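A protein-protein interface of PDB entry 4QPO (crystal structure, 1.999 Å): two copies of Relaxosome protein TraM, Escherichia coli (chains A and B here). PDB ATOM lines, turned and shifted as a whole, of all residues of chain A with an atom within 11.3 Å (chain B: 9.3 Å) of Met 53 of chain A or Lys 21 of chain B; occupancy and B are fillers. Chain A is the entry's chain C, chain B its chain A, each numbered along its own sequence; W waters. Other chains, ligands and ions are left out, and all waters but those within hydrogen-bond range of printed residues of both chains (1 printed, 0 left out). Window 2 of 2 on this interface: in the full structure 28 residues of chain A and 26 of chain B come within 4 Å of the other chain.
NZ of Lys 21 of chain B lies within salt-bridge range of OXT of Met 53 of chain A, 3.4 Å away.
NZ of Lys 14 of chain B is in salt-bridge range of OE2 of Glu 50 of chain A.
ND1 of His 49 of chain A is in hydrogen-bond range of SD of Met 53 of chain A (3.8 Å).
Gly 45 of chain A touches Leu 41 of chain B.
Leu 46 of chain A touches Lys 14 of chain B (CD2 to CB, 3.8 Å).
CD1 of Ile 15 of chain B touches CD1 of Leu 46 of chain A (3.8 Å).
Leu 46 of chain A touches Leu 41 of chain B (CD1 to CD1, 3.6 Å).
His 49 of chain A touches Ile 18 of chain B.
Leu 41 of chain B touches His 49 of chain A.
Ile 18 of chain B touches Met 53 of chain A.
Of the printed residues of chain B, Leu 46 of chain A touches Lys 14, Ile 15 and Leu 41.
Arg 47 of chain A touches none of the printed residues of chain B.
No residue of chain A comes within 4 Å of Ala 17 of chain B.
Ile 18 of chain B touches just these residues of chain A: His 49 and Met 53.
Lys 21 of chain B touches just one residue of chain A: Met 53 (3.4 Å).
No residue of chain A comes within 4 Å of Arg 23 of chain B.
No residue of chain A comes within 4 Å of Glu 25 of chain B.
Of the printed residues of chain A, Leu 41 of chain B touches Gly 45 (3.3 Å), Leu 46 (3.6 Å) and His 49 (3.8 Å).
The nearest residue of chain B that does not touch Met 53 of chain A is Ala 17 of chain B (5.3 Å).
Hydrophobic or aromatic side chains of chain B within 4 Å of the printed part of chain A: Ile 15, Ile 18 and Leu 41.
Among the printed residues, 9 pairs touch across the chains.
Among the printed residues, Asp or Glu carboxylates within 4 Å of a Lys or Arg side-chain nitrogen of the other chain: Glu 50 of chain A with Lys 14 of chain B (3.7 Å).
No position is printed for both chains.
Water W1 lies within hydrogen-bond range of NZ of Lys 21 of chain B (2.7 Å) and OXT of Met 53 of chain A (3.0 Å).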
ATOM      1  N   LEU A  44      -1.571  15.293  15.262  1.00  0.00           N
ATOM      2  CA  LEU A  44      -2.781  14.606  14.834  1.00  0.00           C
ATOM      3  C   LEU A  44      -3.325  13.733  15.965  1.00  0.00           C
ATOM      4  O   LEU A  44      -4.517  13.727  16.237  1.00  0.00           O
ATOM      5  CB  LEU A  44      -2.505  13.762  13.579  1.00  0.00           C
ATOM      6  CG  LEU A  44      -3.608  12.847  13.064  1.00  0.00           C
ATOM      7  CD1 LEU A  44      -4.914  13.612  12.812  1.00  0.00           C
ATOM      8  CD2 LEU A  44      -3.128  12.154  11.775  1.00  0.00           C
ATOM      9  N   GLY A  45      -2.434  13.006  16.629  1.00  0.00           N
ATOM     10  CA  GLY A  45      -2.822  12.153  17.723  1.00  0.00           C
ATOM     11  C   GLY A  45      -3.390  12.984  18.856  1.00  0.00           C
ATOM     12  O   GLY A  45      -4.318  12.550  19.552  1.00  0.00           O
ATOM     13  N   LEU A  46      -2.843  14.181  19.037  1.00  0.00           N
ATOM     14  CA  LEU A  46      -3.346  15.077  20.055  1.00  0.00           C
ATOM     15  C   LEU A  46      -4.761  15.599  19.747  1.00  0.00           C
ATOM     16  O   LEU A  46      -5.615  15.643  20.639  1.00  0.00           O
ATOM     17  CB  LEU A  46      -2.387  16.246  20.224  1.00  0.00           C
ATOM     18  CG  LEU A  46      -2.601  17.168  21.411  1.00  0.00           C
ATOM     19  CD1 LEU A  46      -2.556  16.409  22.721  1.00  0.00           C
ATOM     20  CD2 LEU A  46      -1.516  18.226  21.370  1.00  0.00           C
ATOM     21  N   ARG A  47      -5.011  15.991  18.496  1.00  0.00           N
ATOM     22  CA  ARG A  47      -6.343  16.464  18.116  1.00  0.00           C
ATOM     23  C   ARG A  47      -7.380  15.350  18.326  1.00  0.00           C
ATOM     24  O   ARG A  47      -8.487  15.602  18.749  1.00  0.00           O
ATOM     25  CB  ARG A  47      -6.352  16.945  16.652  1.00  0.00           C
ATOM     26  N   VAL A  48      -7.011  14.109  18.027  1.00  0.00           N
ATOM     27  CA  VAL A  48      -7.920  12.974  18.177  1.00  0.00           C
ATOM     28  C   VAL A  48      -8.234  12.690  19.638  1.00  0.00           C
ATOM     29  O   VAL A  48      -9.389  12.517  20.016  1.00  0.00           O
ATOM     30  CB  VAL A  48      -7.329  11.713  17.534  1.00  0.00           C
ATOM     31  CG1 VAL A  48      -7.951  10.443  18.117  1.00  0.00           C
ATOM     32  CG2 VAL A  48      -7.505  11.782  16.028  1.00  0.00           C
ATOM     33  N   HIS A  49      -7.186  12.635  20.447  1.00  0.00           N
ATOM     34  CA  HIS A  49      -7.335  12.325  21.861  1.00  0.00           C
ATOM     35  C   HIS A  49      -8.214  13.375  22.544  1.00  0.00           C
ATOM     36  O   HIS A  49      -9.037  13.056  23.414  1.00  0.00           O
ATOM     37  CB  HIS A  49      -5.957  12.239  22.523  1.00  0.00           C
ATOM     38  CG  HIS A  49      -5.991  11.697  23.916  1.00  0.00           C
ATOM     39  ND1 HIS A  49      -5.951  12.505  25.031  1.00  0.00           N
ATOM     40  CD2 HIS A  49      -6.048  10.424  24.375  1.00  0.00           C
ATOM     41  CE1 HIS A  49      -5.993  11.756  26.118  1.00  0.00           C
ATOM     42  NE2 HIS A  49      -6.048  10.489  25.747  1.00  0.00           N
ATOM     43  N   GLU A  50      -8.071  14.626  22.108  1.00  0.00           N
ATOM     44  CA  GLU A  50      -8.877  15.729  22.636  1.00  0.00           C
ATOM     45  C   GLU A  50     -10.392  15.576  22.444  1.00  0.00           C
ATOM     46  O   GLU A  50     -11.169  16.209  23.151  1.00  0.00           O
ATOM     47  CB  GLU A  50      -8.439  17.043  21.997  1.00  0.00           C
ATOM     48  CG  GLU A  50      -7.184  17.653  22.577  1.00  0.00           C
ATOM     49  CD  GLU A  50      -6.748  18.866  21.779  1.00  0.00           C
ATOM     50  OE1 GLU A  50      -7.617  19.496  21.141  1.00  0.00           O
ATOM     51  OE2 GLU A  50      -5.543  19.174  21.762  1.00  0.00           O
ATOM     52  N   ALA A  51     -10.822  14.756  21.484  1.00  0.00           N
ATOM     53  CA  ALA A  51     -12.260  14.619  21.220  1.00  0.00           C
ATOM     54  C   ALA A  51     -13.003  13.906  22.367  1.00  0.00           C
ATOM     55  O   ALA A  51     -14.226  14.087  22.538  1.00  0.00           O
ATOM     56  CB  ALA A  51     -12.483  13.882  19.897  1.00  0.00           C
ATOM     57  N   GLN A  52     -12.267  13.125  23.155  1.00  0.00           N
ATOM     58  CA  GLN A  52     -12.850  12.394  24.295  1.00  0.00           C
ATOM     59  C   GLN A  52     -12.747  13.148  25.621  1.00  0.00           C
ATOM     60  O   GLN A  52     -13.071  12.610  26.690  1.00  0.00           O
ATOM     61  CB  GLN A  52     -12.181  11.030  24.458  1.00  0.00           C
ATOM     62  CG  GLN A  52     -12.330  10.121  23.258  1.00  0.00           C
ATOM     63  CD  GLN A  52     -13.729  10.150  22.679  1.00  0.00           C
ATOM     64  OE1 GLN A  52     -13.941  10.693  21.593  1.00  0.00           O
ATOM     65  NE2 GLN A  52     -14.692   9.567  23.398  1.00  0.00           N
ATOM     66  N   MET A  53     -12.305  14.398  25.550  1.00  0.00           N
ATOM     67  CA  MET A  53     -12.130  15.205  26.748  1.00  0.00           C
ATOM     68  C   MET A  53     -13.115  16.374  26.828  1.00  0.00           C
ATOM     69  O   MET A  53     -13.743  16.758  25.832  1.00  0.00           O
ATOM     70  CB  MET A  53     -10.696  15.710  26.810  1.00  0.00           C
ATOM     71  CG  MET A  53      -9.700  14.583  26.947  1.00  0.00           C
ATOM     72  SD  MET A  53      -7.997  15.130  26.777  1.00  0.00           S
ATOM     73  CE  MET A  53      -7.852  16.432  28.003  1.00  0.00           C
ATOM     74  OXT MET A  53     -13.293  16.954  27.904  1.00  0.00           O
ATOM     75  N   GLU B  13       1.927  22.497  25.870  1.00  0.00           N
ATOM     76  CA  GLU B  13       0.974  22.774  26.954  1.00  0.00           C
ATOM     77  C   GLU B  13      -0.128  21.717  27.073  1.00  0.00           C
ATOM     78  O   GLU B  13      -0.463  21.286  28.181  1.00  0.00           O
ATOM     79  CB  GLU B  13       0.330  24.151  26.762  1.00  0.00           C
ATOM     80  CG  GLU B  13       1.239  25.328  27.067  1.00  0.00           C
ATOM     81  CD  GLU B  13       0.581  26.667  26.767  1.00  0.00           C
ATOM     82  OE1 GLU B  13      -0.501  26.682  26.137  1.00  0.00           O
ATOM     83  OE2 GLU B  13       1.151  27.706  27.160  1.00  0.00           O
ATOM     84  N   LYS B  14      -0.697  21.321  25.936  1.00  0.00           N
ATOM     85  CA  LYS B  14      -1.781  20.345  25.918  1.00  0.00           C
ATOM     86  C   LYS B  14      -1.318  18.994  26.470  1.00  0.00           C
ATOM     87  O   LYS B  14      -2.086  18.306  27.141  1.00  0.00           O
ATOM     88  CB  LYS B  14      -2.344  20.164  24.496  1.00  0.00           C
ATOM     89  CG  LYS B  14      -3.026  21.389  23.896  1.00  0.00           C
ATOM     90  CD  LYS B  14      -4.369  21.651  24.546  1.00  0.00           C
ATOM     91  CE  LYS B  14      -5.255  20.403  24.517  1.00  0.00           C
ATOM     92  NZ  LYS B  14      -6.676  20.708  24.878  1.00  0.00           N
ATOM     93  N   ILE B  15      -0.076  18.605  26.183  1.00  0.00           N
ATOM     94  CA  ILE B  15       0.464  17.365  26.741  1.00  0.00           C
ATOM     95  C   ILE B  15       0.504  17.415  28.271  1.00  0.00           C
ATOM     96  O   ILE B  15       0.169  16.441  28.940  1.00  0.00           O
ATOM     97  CB  ILE B  15       1.893  17.057  26.253  1.00  0.00           C
ATOM     98  CG1 ILE B  15       2.037  17.306  24.753  1.00  0.00           C
ATOM     99  CG2 ILE B  15       2.267  15.624  26.622  1.00  0.00           C
ATOM    100  CD1 ILE B  15       1.072  16.533  23.941  1.00  0.00           C
ATOM    101  N   ASN B  16       0.942  18.543  28.814  1.00  0.00           N
ATOM    102  CA  ASN B  16       0.967  18.727  30.261  1.00  0.00           C
ATOM    103  C   ASN B  16      -0.403  18.552  30.893  1.00  0.00           C
ATOM    104  O   ASN B  16      -0.534  17.922  31.941  1.00  0.00           O
ATOM    105  CB  ASN B  16       1.518  20.101  30.606  1.00  0.00           C
ATOM    106  CG  ASN B  16       3.017  20.171  30.456  1.00  0.00           C
ATOM    107  OD1 ASN B  16       3.693  19.144  30.444  1.00  0.00           O
ATOM    108  ND2 ASN B  16       3.553  21.390  30.366  1.00  0.00           N
ATOM    109  N   ALA B  17      -1.422  19.119  30.251  1.00  0.00           N
ATOM    110  CA  ALA B  17      -2.793  19.022  30.746  1.00  0.00           C
ATOM    111  C   ALA B  17      -3.288  17.573  30.703  1.00  0.00           C
ATOM    112  O   ALA B  17      -4.046  17.146  31.569  1.00  0.00           O
ATOM    113  CB  ALA B  17      -3.710  19.920  29.942  1.00  0.00           C
ATOM    114  N   ILE B  18      -2.856  16.822  29.695  1.00  0.00           N
ATOM    115  CA  ILE B  18      -3.179  15.402  29.632  1.00  0.00           C
ATOM    116  C   ILE B  18      -2.617  14.728  30.861  1.00  0.00           C
ATOM    117  O   ILE B  18      -3.336  14.030  31.563  1.00  0.00           O
ATOM    118  CB  ILE B  18      -2.607  14.703  28.382  1.00  0.00           C
ATOM    119  CG1 ILE B  18      -3.141  15.340  27.103  1.00  0.00           C
ATOM    120  CG2 ILE B  18      -2.944  13.211  28.404  1.00  0.00           C
ATOM    121  CD1 ILE B  18      -4.590  15.100  26.890  1.00  0.00           C
ATOM    122  N   ILE B  19      -1.328  14.959  31.104  1.00  0.00           N
ATOM    123  CA  ILE B  19      -0.623  14.429  32.267  1.00  0.00           C
ATOM    124  C   ILE B  19      -1.404  14.682  33.563  1.00  0.00           C
ATOM    125  O   ILE B  19      -1.596  13.773  34.371  1.00  0.00           O
ATOM    126  CB  ILE B  19       0.789  15.055  32.399  1.00  0.00           C
ATOM    127  CG1 ILE B  19       1.670  14.677  31.204  1.00  0.00           C
ATOM    128  CG2 ILE B  19       1.442  14.627  33.705  1.00  0.00           C
ATOM    129  CD1 ILE B  19       3.019  15.366  31.199  1.00  0.00           C
ATOM    130  N   GLU B  20      -1.863  15.920  33.735  1.00  0.00           N
ATOM    131  CA  GLU B  20      -2.598  16.329  34.932  1.00  0.00           C
ATOM    132  C   GLU B  20      -3.949  15.627  35.061  1.00  0.00           C
ATOM    133  O   GLU B  20      -4.320  15.166  36.143  1.00  0.00           O
ATOM    134  CB  GLU B  20      -2.805  17.846  34.931  1.00  0.00           C
ATOM    135  CG  GLU B  20      -1.638  18.635  35.486  1.00  0.00           C
ATOM    136  CD  GLU B  20      -1.556  18.568  37.002  1.00  0.00           C
ATOM    137  OE1 GLU B  20      -2.559  18.172  37.641  1.00  0.00           O
ATOM    138  OE2 GLU B  20      -0.491  18.913  37.558  1.00  0.00           O
ATOM    139  N   LYS B  21      -4.682  15.565  33.955  1.00  0.00           N
ATOM    140  CA  LYS B  21      -6.001  14.937  33.927  1.00  0.00           C
ATOM    141  C   LYS B  21      -5.909  13.433  34.199  1.00  0.00           C
ATOM    142  O   LYS B  21      -6.813  12.842  34.800  1.00  0.00           O
ATOM    143  CB  LYS B  21      -6.679  15.199  32.579  1.00  0.00           C
ATOM    144  CG  LYS B  21      -8.130  14.756  32.500  1.00  0.00           C
ATOM    145  CD  LYS B  21      -8.795  15.315  31.254  1.00  0.00           C
ATOM    146  CE  LYS B  21     -10.295  15.066  31.263  1.00  0.00           C
ATOM    147  NZ  LYS B  21     -11.016  15.828  30.194  1.00  0.00           N
ATOM    148  N   ARG B  22      -4.814  12.818  33.755  1.00  0.00           N
ATOM    149  CA  ARG B  22      -4.567  11.407  34.029  1.00  0.00           C
ATOM    150  C   ARG B  22      -4.325  11.195  35.520  1.00  0.00           C
ATOM    151  O   ARG B  22      -4.952  10.334  36.133  1.00  0.00           O
ATOM    152  CB  ARG B  22      -3.376  10.888  33.222  1.00  0.00           C
ATOM    153  CG  ARG B  22      -3.536  10.971  31.706  1.00  0.00           C
ATOM    154  CD  ARG B  22      -4.092   9.693  31.107  1.00  0.00           C
ATOM    155  NE  ARG B  22      -3.505   9.397  29.799  1.00  0.00           N
ATOM    156  CZ  ARG B  22      -2.449   8.609  29.617  1.00  0.00           C
ATOM    157  NH1 ARG B  22      -1.866   8.038  30.660  1.00  0.00           N
ATOM    158  NH2 ARG B  22      -1.976   8.386  28.397  1.00  0.00           N
ATOM    159  N   ARG B  23      -3.437  11.996  36.106  1.00  0.00           N
ATOM    160  CA  ARG B  23      -3.134  11.899  37.535  1.00  0.00           C
ATOM    161  C   ARG B  23      -4.358  12.212  38.416  1.00  0.00           C
ATOM    162  O   ARG B  23      -4.328  12.004  39.633  1.00  0.00           O
ATOM    163  CB  ARG B  23      -1.971  12.830  37.896  1.00  0.00           C
ATOM    164  N   GLN B  24      -5.425  12.713  37.796  1.00  0.00           N
ATOM    165  CA  GLN B  24      -6.697  12.943  38.482  1.00  0.00           C
ATOM    166  C   GLN B  24      -7.744  11.886  38.108  1.00  0.00           C
ATOM    167  O   GLN B  24      -8.847  11.875  38.660  1.00  0.00           O
ATOM    168  CB  GLN B  24      -7.243  14.342  38.164  1.00  0.00           C
ATOM    169  CG  GLN B  24      -6.320  15.491  38.536  1.00  0.00           C
ATOM    170  CD  GLN B  24      -5.856  15.430  39.978  1.00  0.00           C
ATOM    171  OE1 GLN B  24      -4.655  15.366  40.253  1.00  0.00           O
ATOM    172  NE2 GLN B  24      -6.803  15.455  40.907  1.00  0.00           N
ATOM    173  N   GLU B  25      -7.400  11.003  37.175  1.00  0.00           N
ATOM    174  CA  GLU B  25      -8.339   9.991  36.699  1.00  0.00           C
ATOM    175  C   GLU B  25      -7.738   8.578  36.695  1.00  0.00           C
ATOM    176  O   GLU B  25      -7.562   7.977  35.634  1.00  0.00           O
ATOM    177  CB  GLU B  25      -8.835  10.353  35.293  1.00  0.00           C
ATOM    178  N   GLY B  26      -7.426   8.056  37.882  1.00  0.00           N
ATOM    179  CA  GLY B  26      -6.906   6.704  38.030  1.00  0.00           C
ATOM    180  C   GLY B  26      -5.490   6.473  37.524  1.00  0.00           C
ATOM    181  O   GLY B  26      -5.240   5.517  36.792  1.00  0.00           O
ATOM    182  N   ALA B  27      -4.561   7.342  37.914  1.00  0.00           N
ATOM    183  CA  ALA B  27      -3.150   7.194  37.543  1.00  0.00           C
ATOM    184  C   ALA B  27      -2.245   7.675  38.679  1.00  0.00           C
ATOM    185  O   ALA B  27      -2.722   8.266  39.649  1.00  0.00           O
ATOM    186  CB  ALA B  27      -2.848   7.951  36.257  1.00  0.00           C
ATOM    187  N   ARG B  28      -0.945   7.419  38.562  1.00  0.00           N
ATOM    188  CA  ARG B  28      -0.007   7.725  39.640  1.00  0.00           C
ATOM    189  C   ARG B  28       1.151   8.611  39.182  1.00  0.00           C
ATOM    190  O   ARG B  28       1.391   8.764  37.984  1.00  0.00           O
ATOM    191  CB  ARG B  28       0.547   6.428  40.238  1.00  0.00           C
ATOM    192  N   VAL B  32       2.685   8.251  33.628  1.00  0.00           N
ATOM    193  CA  VAL B  32       2.119   9.277  32.737  1.00  0.00           C
ATOM    194  C   VAL B  32       3.103  10.439  32.493  1.00  0.00           C
ATOM    195  O   VAL B  32       2.714  11.589  32.260  1.00  0.00           O
ATOM    196  CB  VAL B  32       0.723   9.804  33.249  1.00  0.00           C
ATOM    197  CG1 VAL B  32       0.818  10.888  34.341  1.00  0.00           C
ATOM    198  CG2 VAL B  32      -0.097  10.309  32.078  1.00  0.00           C
ATOM    199  N   THR B  37       3.484   9.911  27.217  1.00  0.00           N
ATOM    200  CA  THR B  37       2.273  10.474  26.647  1.00  0.00           C
ATOM    201  C   THR B  37       2.512  10.958  25.219  1.00  0.00           C
ATOM    202  O   THR B  37       1.724  10.663  24.320  1.00  0.00           O
ATOM    203  CB  THR B  37       1.744  11.632  27.522  1.00  0.00           C
ATOM    204  OG1 THR B  37       1.281  11.090  28.755  1.00  0.00           O
ATOM    205  CG2 THR B  37       0.586  12.345  26.853  1.00  0.00           C
ATOM    206  N   LEU B  41       0.895   9.552  21.815  1.00  0.00           N
ATOM    207  CA  LEU B  41       0.132  10.387  20.906  1.00  0.00           C
ATOM    208  C   LEU B  41       0.659  10.293  19.476  1.00  0.00           C
ATOM    209  O   LEU B  41      -0.119  10.397  18.513  1.00  0.00           O
ATOM    210  CB  LEU B  41       0.140  11.832  21.384  1.00  0.00           C
ATOM    211  CG  LEU B  41      -0.727  12.146  22.597  1.00  0.00           C
ATOM    212  CD1 LEU B  41      -0.403  13.532  23.059  1.00  0.00           C
ATOM    213  CD2 LEU B  41      -2.214  12.023  22.247  1.00  0.00           C
HETATM  214  O   HOH W   1     -11.860  18.376  30.161  1.00  0.00           O
